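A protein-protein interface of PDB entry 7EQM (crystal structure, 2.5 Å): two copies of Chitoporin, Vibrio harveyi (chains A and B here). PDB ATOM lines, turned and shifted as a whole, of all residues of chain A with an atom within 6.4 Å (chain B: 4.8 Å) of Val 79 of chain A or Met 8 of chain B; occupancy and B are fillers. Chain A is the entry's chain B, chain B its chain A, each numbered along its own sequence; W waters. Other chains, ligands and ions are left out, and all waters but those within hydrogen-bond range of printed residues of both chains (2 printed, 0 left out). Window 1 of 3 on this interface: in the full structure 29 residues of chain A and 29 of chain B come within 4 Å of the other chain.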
ATOM      1  N   PHE A  52      -9.659   1.858  18.463  1.00  0.00           N
ATOM      2  CA  PHE A  52      -9.718   0.417  18.307  1.00  0.00           C
ATOM      3  C   PHE A  52     -10.253   0.108  16.919  1.00  0.00           C
ATOM      4  O   PHE A  52     -11.219   0.734  16.468  1.00  0.00           O
ATOM      5  CB  PHE A  52     -10.603  -0.194  19.398  1.00  0.00           C
ATOM      6  CG  PHE A  52     -10.608  -1.702  19.422  1.00  0.00           C
ATOM      7  CD1 PHE A  52      -9.434  -2.418  19.629  1.00  0.00           C
ATOM      8  CD2 PHE A  52     -11.805  -2.404  19.261  1.00  0.00           C
ATOM      9  CE1 PHE A  52      -9.443  -3.808  19.660  1.00  0.00           C
ATOM     10  CE2 PHE A  52     -11.833  -3.797  19.298  1.00  0.00           C
ATOM     11  CZ  PHE A  52     -10.645  -4.500  19.499  1.00  0.00           C
ATOM     12  N   ILE A  53      -9.605  -0.830  16.229  1.00  0.00           N
ATOM     13  CA  ILE A  53     -10.101  -1.349  14.961  1.00  0.00           C
ATOM     14  C   ILE A  53     -10.154  -2.867  15.056  1.00  0.00           C
ATOM     15  O   ILE A  53      -9.454  -3.486  15.863  1.00  0.00           O
ATOM     16  CB  ILE A  53      -9.231  -0.904  13.769  1.00  0.00           C
ATOM     17  CG1 ILE A  53      -7.833  -1.530  13.858  1.00  0.00           C
ATOM     18  CG2 ILE A  53      -9.128   0.617  13.722  1.00  0.00           C
ATOM     19  CD1 ILE A  53      -6.818  -0.894  12.929  1.00  0.00           C
ATOM     20  N   TRP A  54     -11.019  -3.467  14.235  1.00  0.00           N
ATOM     21  CA  TRP A  54     -11.124  -4.919  14.185  1.00  0.00           C
ATOM     22  C   TRP A  54     -11.804  -5.349  12.886  1.00  0.00           C
ATOM     23  O   TRP A  54     -12.617  -4.611  12.318  1.00  0.00           O
ATOM     24  CB  TRP A  54     -11.884  -5.453  15.399  1.00  0.00           C
ATOM     25  CG  TRP A  54     -13.328  -5.079  15.402  1.00  0.00           C
ATOM     26  CD1 TRP A  54     -13.896  -4.000  16.017  1.00  0.00           C
ATOM     27  CD2 TRP A  54     -14.389  -5.766  14.732  1.00  0.00           C
ATOM     28  NE1 TRP A  54     -15.246  -3.979  15.778  1.00  0.00           N
ATOM     29  CE2 TRP A  54     -15.577  -5.053  14.994  1.00  0.00           C
ATOM     30  CE3 TRP A  54     -14.448  -6.909  13.931  1.00  0.00           C
ATOM     31  CZ2 TRP A  54     -16.814  -5.446  14.490  1.00  0.00           C
ATOM     32  CZ3 TRP A  54     -15.676  -7.304  13.432  1.00  0.00           C
ATOM     33  CH2 TRP A  54     -16.847  -6.574  13.720  1.00  0.00           C
ATOM     34  N   GLN A  55     -11.470  -6.562  12.432  1.00  0.00           N
ATOM     35  CA  GLN A  55     -12.005  -7.125  11.199  1.00  0.00           C
ATOM     36  C   GLN A  55     -12.093  -8.637  11.339  1.00  0.00           C
ATOM     37  O   GLN A  55     -11.196  -9.258  11.910  1.00  0.00           O
ATOM     38  CB  GLN A  55     -11.135  -6.774   9.983  1.00  0.00           C
ATOM     39  CG  GLN A  55     -11.727  -7.182   8.636  1.00  0.00           C
ATOM     40  CD  GLN A  55     -10.890  -6.720   7.452  1.00  0.00           C
ATOM     41  OE1 GLN A  55     -10.994  -5.575   7.018  1.00  0.00           O
ATOM     42  NE2 GLN A  55     -10.059  -7.613   6.919  1.00  0.00           N
ATOM     43  N   THR A  77      -8.180 -11.249   9.539  1.00  0.00           N
ATOM     44  CA  THR A  77      -9.012 -11.217  10.736  1.00  0.00           C
ATOM     45  C   THR A  77      -8.136 -10.779  11.896  1.00  0.00           C
ATOM     46  O   THR A  77      -7.188 -11.485  12.250  1.00  0.00           O
ATOM     47  CB  THR A  77      -9.632 -12.581  10.989  1.00  0.00           C
ATOM     48  OG1 THR A  77     -10.493 -12.883   9.888  1.00  0.00           O
ATOM     49  CG2 THR A  77     -10.432 -12.583  12.303  1.00  0.00           C
ATOM     50  N   PHE A  78      -8.437  -9.620  12.485  1.00  0.00           N
ATOM     51  CA  PHE A  78      -7.473  -8.991  13.387  1.00  0.00           C
ATOM     52  C   PHE A  78      -8.185  -8.031  14.331  1.00  0.00           C
ATOM     53  O   PHE A  78      -9.383  -7.762  14.202  1.00  0.00           O
ATOM     54  CB  PHE A  78      -6.392  -8.239  12.600  1.00  0.00           C
ATOM     55  CG  PHE A  78      -6.947  -7.203  11.671  1.00  0.00           C
ATOM     56  CD1 PHE A  78      -7.306  -5.933  12.148  1.00  0.00           C
ATOM     57  CD2 PHE A  78      -7.120  -7.490  10.312  1.00  0.00           C
ATOM     58  CE1 PHE A  78      -7.838  -4.973  11.284  1.00  0.00           C
ATOM     59  CE2 PHE A  78      -7.646  -6.536   9.434  1.00  0.00           C
ATOM     60  CZ  PHE A  78      -8.007  -5.278   9.919  1.00  0.00           C
ATOM     61  N   VAL A  79      -7.403  -7.493  15.266  1.00  0.00           N
ATOM     62  CA  VAL A  79      -7.746  -6.342  16.086  1.00  0.00           C
ATOM     63  C   VAL A  79      -6.544  -5.414  16.062  1.00  0.00           C
ATOM     64  O   VAL A  79      -5.410  -5.832  15.806  1.00  0.00           O
ATOM     65  CB  VAL A  79      -8.087  -6.735  17.537  1.00  0.00           C
ATOM     66  CG1 VAL A  79      -9.113  -7.836  17.538  1.00  0.00           C
ATOM     67  CG2 VAL A  79      -6.844  -7.218  18.260  1.00  0.00           C
ATOM     68  N   GLY A  80      -6.785  -4.143  16.340  1.00  0.00           N
ATOM     69  CA  GLY A  80      -5.651  -3.249  16.367  1.00  0.00           C
ATOM     70  C   GLY A  80      -6.002  -1.892  16.920  1.00  0.00           C
ATOM     71  O   GLY A  80      -7.091  -1.671  17.455  1.00  0.00           O
ATOM     72  N   PHE A  81      -5.039  -0.988  16.783  1.00  0.00           N
ATOM     73  CA  PHE A  81      -5.205   0.407  17.150  1.00  0.00           C
ATOM     74  C   PHE A  81      -4.597   1.263  16.048  1.00  0.00           C
ATOM     75  O   PHE A  81      -3.679   0.836  15.342  1.00  0.00           O
ATOM     76  CB  PHE A  81      -4.560   0.715  18.511  1.00  0.00           C
ATOM     77  CG  PHE A  81      -5.247   0.042  19.678  1.00  0.00           C
ATOM     78  CD1 PHE A  81      -6.401   0.585  20.229  1.00  0.00           C
ATOM     79  CD2 PHE A  81      -4.742  -1.138  20.209  1.00  0.00           C
ATOM     80  CE1 PHE A  81      -7.042  -0.042  21.296  1.00  0.00           C
ATOM     81  CE2 PHE A  81      -5.367  -1.767  21.262  1.00  0.00           C
ATOM     82  CZ  PHE A  81      -6.516  -1.220  21.815  1.00  0.00           C
ATOM     83  N   VAL A  89      -1.481  -0.543  14.039  1.00  0.00           N
ATOM     84  CA  VAL A  89      -0.959  -1.830  14.444  1.00  0.00           C
ATOM     85  C   VAL A  89      -2.118  -2.808  14.434  1.00  0.00           C
ATOM     86  O   VAL A  89      -3.237  -2.469  14.840  1.00  0.00           O
ATOM     87  CB  VAL A  89      -0.283  -1.756  15.826  1.00  0.00           C
ATOM     88  CG1 VAL A  89       0.420  -3.069  16.148  1.00  0.00           C
ATOM     89  CG2 VAL A  89       0.720  -0.637  15.813  1.00  0.00           C
ATOM     90  N   ARG A  90      -1.851  -4.008  13.930  1.00  0.00           N
ATOM     91  CA  ARG A  90      -2.846  -5.051  13.780  1.00  0.00           C
ATOM     92  C   ARG A  90      -2.273  -6.319  14.370  1.00  0.00           C
ATOM     93  O   ARG A  90      -1.136  -6.681  14.056  1.00  0.00           O
ATOM     94  CB  ARG A  90      -3.198  -5.270  12.311  1.00  0.00           C
ATOM     95  CG  ARG A  90      -4.159  -4.263  11.755  1.00  0.00           C
ATOM     96  CD  ARG A  90      -4.548  -4.615  10.322  1.00  0.00           C
ATOM     97  NE  ARG A  90      -3.420  -4.438   9.419  1.00  0.00           N
ATOM     98  CZ  ARG A  90      -3.397  -4.880   8.165  1.00  0.00           C
ATOM     99  NH1 ARG A  90      -4.447  -5.521   7.666  1.00  0.00           N
ATOM    100  NH2 ARG A  90      -2.322  -4.684   7.409  1.00  0.00           N
ATOM    101  N   LEU A  91      -3.041  -6.980  15.230  1.00  0.00           N
ATOM    102  CA  LEU A  91      -2.692  -8.309  15.710  1.00  0.00           C
ATOM    103  C   LEU A  91      -3.687  -9.297  15.136  1.00  0.00           C
ATOM    104  O   LEU A  91      -4.898  -9.083  15.231  1.00  0.00           O
ATOM    105  CB  LEU A  91      -2.723  -8.420  17.236  1.00  0.00           C
ATOM    106  CG  LEU A  91      -2.056  -7.374  18.119  1.00  0.00           C
ATOM    107  CD1 LEU A  91      -1.745  -7.988  19.475  1.00  0.00           C
ATOM    108  CD2 LEU A  91      -0.816  -6.847  17.479  1.00  0.00           C
ATOM    109  N   GLY A  92      -3.180 -10.376  14.553  1.00  0.00           N
ATOM    110  CA  GLY A  92      -4.058 -11.451  14.155  1.00  0.00           C
ATOM    111  C   GLY A  92      -3.597 -12.163  12.911  1.00  0.00           C
ATOM    112  O   GLY A  92      -2.442 -12.580  12.800  1.00  0.00           O
ATOM    113  N   ILE B   6     -15.369  -9.274  20.314  1.00  0.00           N
ATOM    114  CA  ILE B   6     -14.045  -9.218  19.716  1.00  0.00           C
ATOM    115  C   ILE B   6     -13.050  -9.424  20.848  1.00  0.00           C
ATOM    116  O   ILE B   6     -12.952  -8.587  21.749  1.00  0.00           O
ATOM    117  CB  ILE B   6     -13.805  -7.890  18.983  1.00  0.00           C
ATOM    118  CG1 ILE B   6     -14.902  -7.634  17.939  1.00  0.00           C
ATOM    119  CG2 ILE B   6     -12.459  -7.889  18.335  1.00  0.00           C
ATOM    120  CD1 ILE B   6     -15.237  -8.827  17.077  1.00  0.00           C
ATOM    121  N   ALA B   7     -12.324 -10.543  20.815  1.00  0.00           N
ATOM    122  CA  ALA B   7     -11.444 -10.954  21.907  1.00  0.00           C
ATOM    123  C   ALA B   7     -10.103 -11.380  21.342  1.00  0.00           C
ATOM    124  O   ALA B   7     -10.038 -12.245  20.462  1.00  0.00           O
ATOM    125  CB  ALA B   7     -12.048 -12.106  22.728  1.00  0.00           C
ATOM    126  N   MET B   8      -9.036 -10.793  21.863  1.00  0.00           N
ATOM    127  CA  MET B   8      -7.692 -11.079  21.380  1.00  0.00           C
ATOM    128  C   MET B   8      -6.751 -11.160  22.569  1.00  0.00           C
ATOM    129  O   MET B   8      -6.624 -10.202  23.337  1.00  0.00           O
ATOM    130  CB  MET B   8      -7.216 -10.000  20.401  1.00  0.00           C
ATOM    131  CG  MET B   8      -5.803 -10.214  19.881  1.00  0.00           C
ATOM    132  SD  MET B   8      -5.720 -11.552  18.665  1.00  0.00           S
ATOM    133  CE  MET B   8      -4.860 -12.736  19.650  1.00  0.00           C
ATOM    134  N   GLN B   9      -6.082 -12.292  22.716  1.00  0.00           N
ATOM    135  CA  GLN B   9      -5.136 -12.477  23.804  1.00  0.00           C
ATOM    136  C   GLN B   9      -3.814 -12.886  23.191  1.00  0.00           C
ATOM    137  O   GLN B   9      -3.760 -13.889  22.475  1.00  0.00           O
ATOM    138  CB  GLN B   9      -5.652 -13.538  24.783  1.00  0.00           C
ATOM    139  CG  GLN B   9      -4.663 -14.042  25.827  1.00  0.00           C
ATOM    140  CD  GLN B   9      -5.261 -15.197  26.637  1.00  0.00           C
ATOM    141  OE1 GLN B   9      -6.129 -15.921  26.148  1.00  0.00           O
ATOM    142  NE2 GLN B   9      -4.822 -15.349  27.880  1.00  0.00           N
ATOM    143  N   ALA B  10      -2.767 -12.096  23.417  1.00  0.00           N
ATOM    144  CA  ALA B  10      -1.413 -12.495  23.030  1.00  0.00           C
ATOM    145  C   ALA B  10      -0.788 -13.226  24.215  1.00  0.00           C
ATOM    146  O   ALA B  10      -0.507 -12.619  25.249  1.00  0.00           O
ATOM    147  CB  ALA B  10      -0.572 -11.289  22.625  1.00  0.00           C
ATOM    148  N   LEU B  31      -1.015 -16.032  19.315  1.00  0.00           N
ATOM    149  CA  LEU B  31      -2.197 -15.188  19.388  1.00  0.00           C
ATOM    150  C   LEU B  31      -3.415 -16.082  19.571  1.00  0.00           C
ATOM    151  O   LEU B  31      -3.586 -17.058  18.832  1.00  0.00           O
ATOM    152  CB  LEU B  31      -2.326 -14.335  18.130  1.00  0.00           C
ATOM    153  CG  LEU B  31      -1.370 -13.140  17.990  1.00  0.00           C
ATOM    154  CD1 LEU B  31      -1.791 -12.236  16.827  1.00  0.00           C
ATOM    155  CD2 LEU B  31      -1.269 -12.341  19.271  1.00  0.00           C
ATOM    156  N   ASN B  32      -4.232 -15.779  20.578  1.00  0.00           N
ATOM    157  CA  ASN B  32      -5.492 -16.478  20.840  1.00  0.00           C
ATOM    158  C   ASN B  32      -6.634 -15.529  20.470  1.00  0.00           C
ATOM    159  O   ASN B  32      -7.000 -14.649  21.258  1.00  0.00           O
ATOM    160  CB  ASN B  32      -5.576 -16.915  22.306  1.00  0.00           C
ATOM    161  CG  ASN B  32      -6.783 -17.827  22.600  1.00  0.00           C
ATOM    162  OD1 ASN B  32      -7.220 -18.621  21.751  1.00  0.00           O
ATOM    163  ND2 ASN B  32      -7.303 -17.729  23.821  1.00  0.00           N
ATOM    164  N   ASN B  33      -7.192 -15.708  19.272  1.00  0.00           N
ATOM    165  CA  ASN B  33      -8.286 -14.868  18.765  1.00  0.00           C
ATOM    166  C   ASN B  33      -9.605 -15.586  19.026  1.00  0.00           C
ATOM    167  O   ASN B  33      -9.974 -16.528  18.319  1.00  0.00           O
ATOM    168  CB  ASN B  33      -8.124 -14.560  17.276  1.00  0.00           C
ATOM    169  CG  ASN B  33      -9.051 -13.451  16.804  1.00  0.00           C
ATOM    170  OD1 ASN B  33      -9.892 -12.965  17.556  1.00  0.00           O
ATOM    171  ND2 ASN B  33      -8.887 -13.030  15.555  1.00  0.00           N
ATOM    172  N   SER B  35     -12.485 -13.906  18.941  1.00  0.00           N
ATOM    173  CA  SER B  35     -13.554 -13.104  18.373  1.00  0.00           C
ATOM    174  C   SER B  35     -14.636 -14.020  17.807  1.00  0.00           C
ATOM    175  O   SER B  35     -14.347 -15.077  17.228  1.00  0.00           O
ATOM    176  CB  SER B  35     -13.016 -12.171  17.280  1.00  0.00           C
ATOM    177  OG  SER B  35     -11.932 -11.390  17.754  1.00  0.00           O
ATOM    178  N   TYR B 291      -6.460  -6.315  29.608  1.00  0.00           N
ATOM    179  CA  TYR B 291      -6.032  -7.091  30.757  1.00  0.00           C
ATOM    180  C   TYR B 291      -4.621  -7.639  30.556  1.00  0.00           C
ATOM    181  O   TYR B 291      -4.119  -7.769  29.437  1.00  0.00           O
ATOM    182  CB  TYR B 291      -7.029  -8.214  31.069  1.00  0.00           C
ATOM    183  CG  TYR B 291      -7.131  -9.301  30.041  1.00  0.00           C
ATOM    184  CD1 TYR B 291      -6.322 -10.434  30.111  1.00  0.00           C
ATOM    185  CD2 TYR B 291      -8.054  -9.217  29.007  1.00  0.00           C
ATOM    186  CE1 TYR B 291      -6.429 -11.454  29.155  1.00  0.00           C
ATOM    187  CE2 TYR B 291      -8.170 -10.231  28.064  1.00  0.00           C
ATOM    188  CZ  TYR B 291      -7.352 -11.336  28.142  1.00  0.00           C
ATOM    189  OH  TYR B 291      -7.460 -12.329  27.200  1.00  0.00           O
ATOM    190  N   VAL B 325      -1.396 -10.574  27.546  1.00  0.00           N
ATOM    191  CA  VAL B 325      -2.212  -9.371  27.549  1.00  0.00           C
ATOM    192  C   VAL B 325      -3.374  -9.602  26.586  1.00  0.00           C
ATOM    193  O   VAL B 325      -3.288 -10.418  25.658  1.00  0.00           O
ATOM    194  CB  VAL B 325      -1.401  -8.125  27.145  1.00  0.00           C
ATOM    195  CG1 VAL B 325      -0.185  -7.967  28.046  1.00  0.00           C
ATOM    196  CG2 VAL B 325      -0.987  -8.215  25.679  1.00  0.00           C
ATOM    197  N   GLY B 326      -4.473  -8.888  26.813  1.00  0.00           N
ATOM    198  CA  GLY B 326      -5.659  -9.100  26.007  1.00  0.00           C
ATOM    199  C   GLY B 326      -6.559  -7.883  25.933  1.00  0.00           C
ATOM    200  O   GLY B 326      -6.478  -6.951  26.750  1.00  0.00           O
ATOM    201  N   VAL B 327      -7.411  -7.905  24.915  1.00  0.00           N
ATOM    202  CA  VAL B 327      -8.493  -6.952  24.736  1.00  0.00           C
ATOM    203  C   VAL B 327      -9.760  -7.750  24.477  1.00  0.00           C
ATOM    204  O   VAL B 327      -9.738  -8.754  23.754  1.00  0.00           O
ATOM    205  CB  VAL B 327      -8.224  -5.974  23.571  1.00  0.00           C
ATOM    206  CG1 VAL B 327      -7.837  -6.735  22.321  1.00  0.00           C
ATOM    207  CG2 VAL B 327      -9.458  -5.105  23.290  1.00  0.00           C
HETATM  208  O   HOH W   1     -10.684 -10.678  15.060  1.00  0.00           O
HETATM  209  O   HOH W   2      -6.569 -13.954  13.760  1.00  0.00           O
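Water W2 lies within hydrogen-bond range of O of Thr 77 of chain A (3.0 Å) and ND2 of Asn 33 of chain B (3.1 Å).
Water W1 lies within hydrogen-bond range of the side-chain amide nitrogen of Asn 33 of chain B (3.0 Å), the side-chain hydroxyl of Ser 35 of chain B (3.1 Å), the backbone carbonyl oxygen of Phe 78 of chain A (3.3 Å) and the backbone carbonyl oxygen of Gln 55 of chain A (3.5 Å).
Of the printed residues of chain B, Trp 54 of chain A touches Ile 6.
Of the printed residues of chain B, Val 79 of chain A touches Ile 6 and Met 8.
Val 89 of chain A touches none of the printed residues of chain B.
Of chain A, only Val 79 comes within 4 Å of Met 8 of chain B.
Of the printed residues of chain A, Leu 31 of chain B touches Leu 91 and Gly 92.
Asn 32 of chain B touches none of the printed residues of chain A.
Among the printed residues, merely in contact across the chains: Phe 52 of chain A with Val 327 of chain B, Trp 54 of chain A with Ile 6 of chain B, Thr 77 of chain A with Asn 33 of chain B, Val 79 of chain A with Ile 6 of chain B, Val 79 of chain A with Met 8 of chain B, Leu 91 of chain A with Leu 31 of chain B and Gly 92 of chain A with Leu 31 of chain B.
Printed residues of chain B that touch a printed residue of chain A: Ile 6, Met 8, Leu 31, Asn 33 and Val 327.
Hydrophobic or aromatic side chains of chain B that line the printed part of chain A: Ile 6, Met 8, Leu 31 and Val 327.
Among the printed residues, 7 pairs touch across the chains.
Among the printed residues, no Asp or Glu carboxylate lies within 4 Å of a Lys or Arg side-chain nitrogen of the other chain.
No position is printed for both chains.
Of the 7 pairs that touch across the chains among the printed residues, none has its exchanged pair printed and touching as well.
O of Ala 7 of chain B lies close to OD1 of Asn 33 of chain B.
The backbone NH (N) of Met 8 of chain B sits at hydrogen-bond distance from the backbone carbonyl oxygen (O) of Val 327 of chain B, 2.9 Å away.
The side-chain hydroxyl (OG) of Ser 35 of chain B is in hydrogen-bond range of the side-chain amide oxygen (OD1) of Asn 33 of chain B, at 2.6 Å.
O of Val 79 of chain A is in hydrogen-bond range of N of Leu 91 of chain A, 2.7 Å away.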
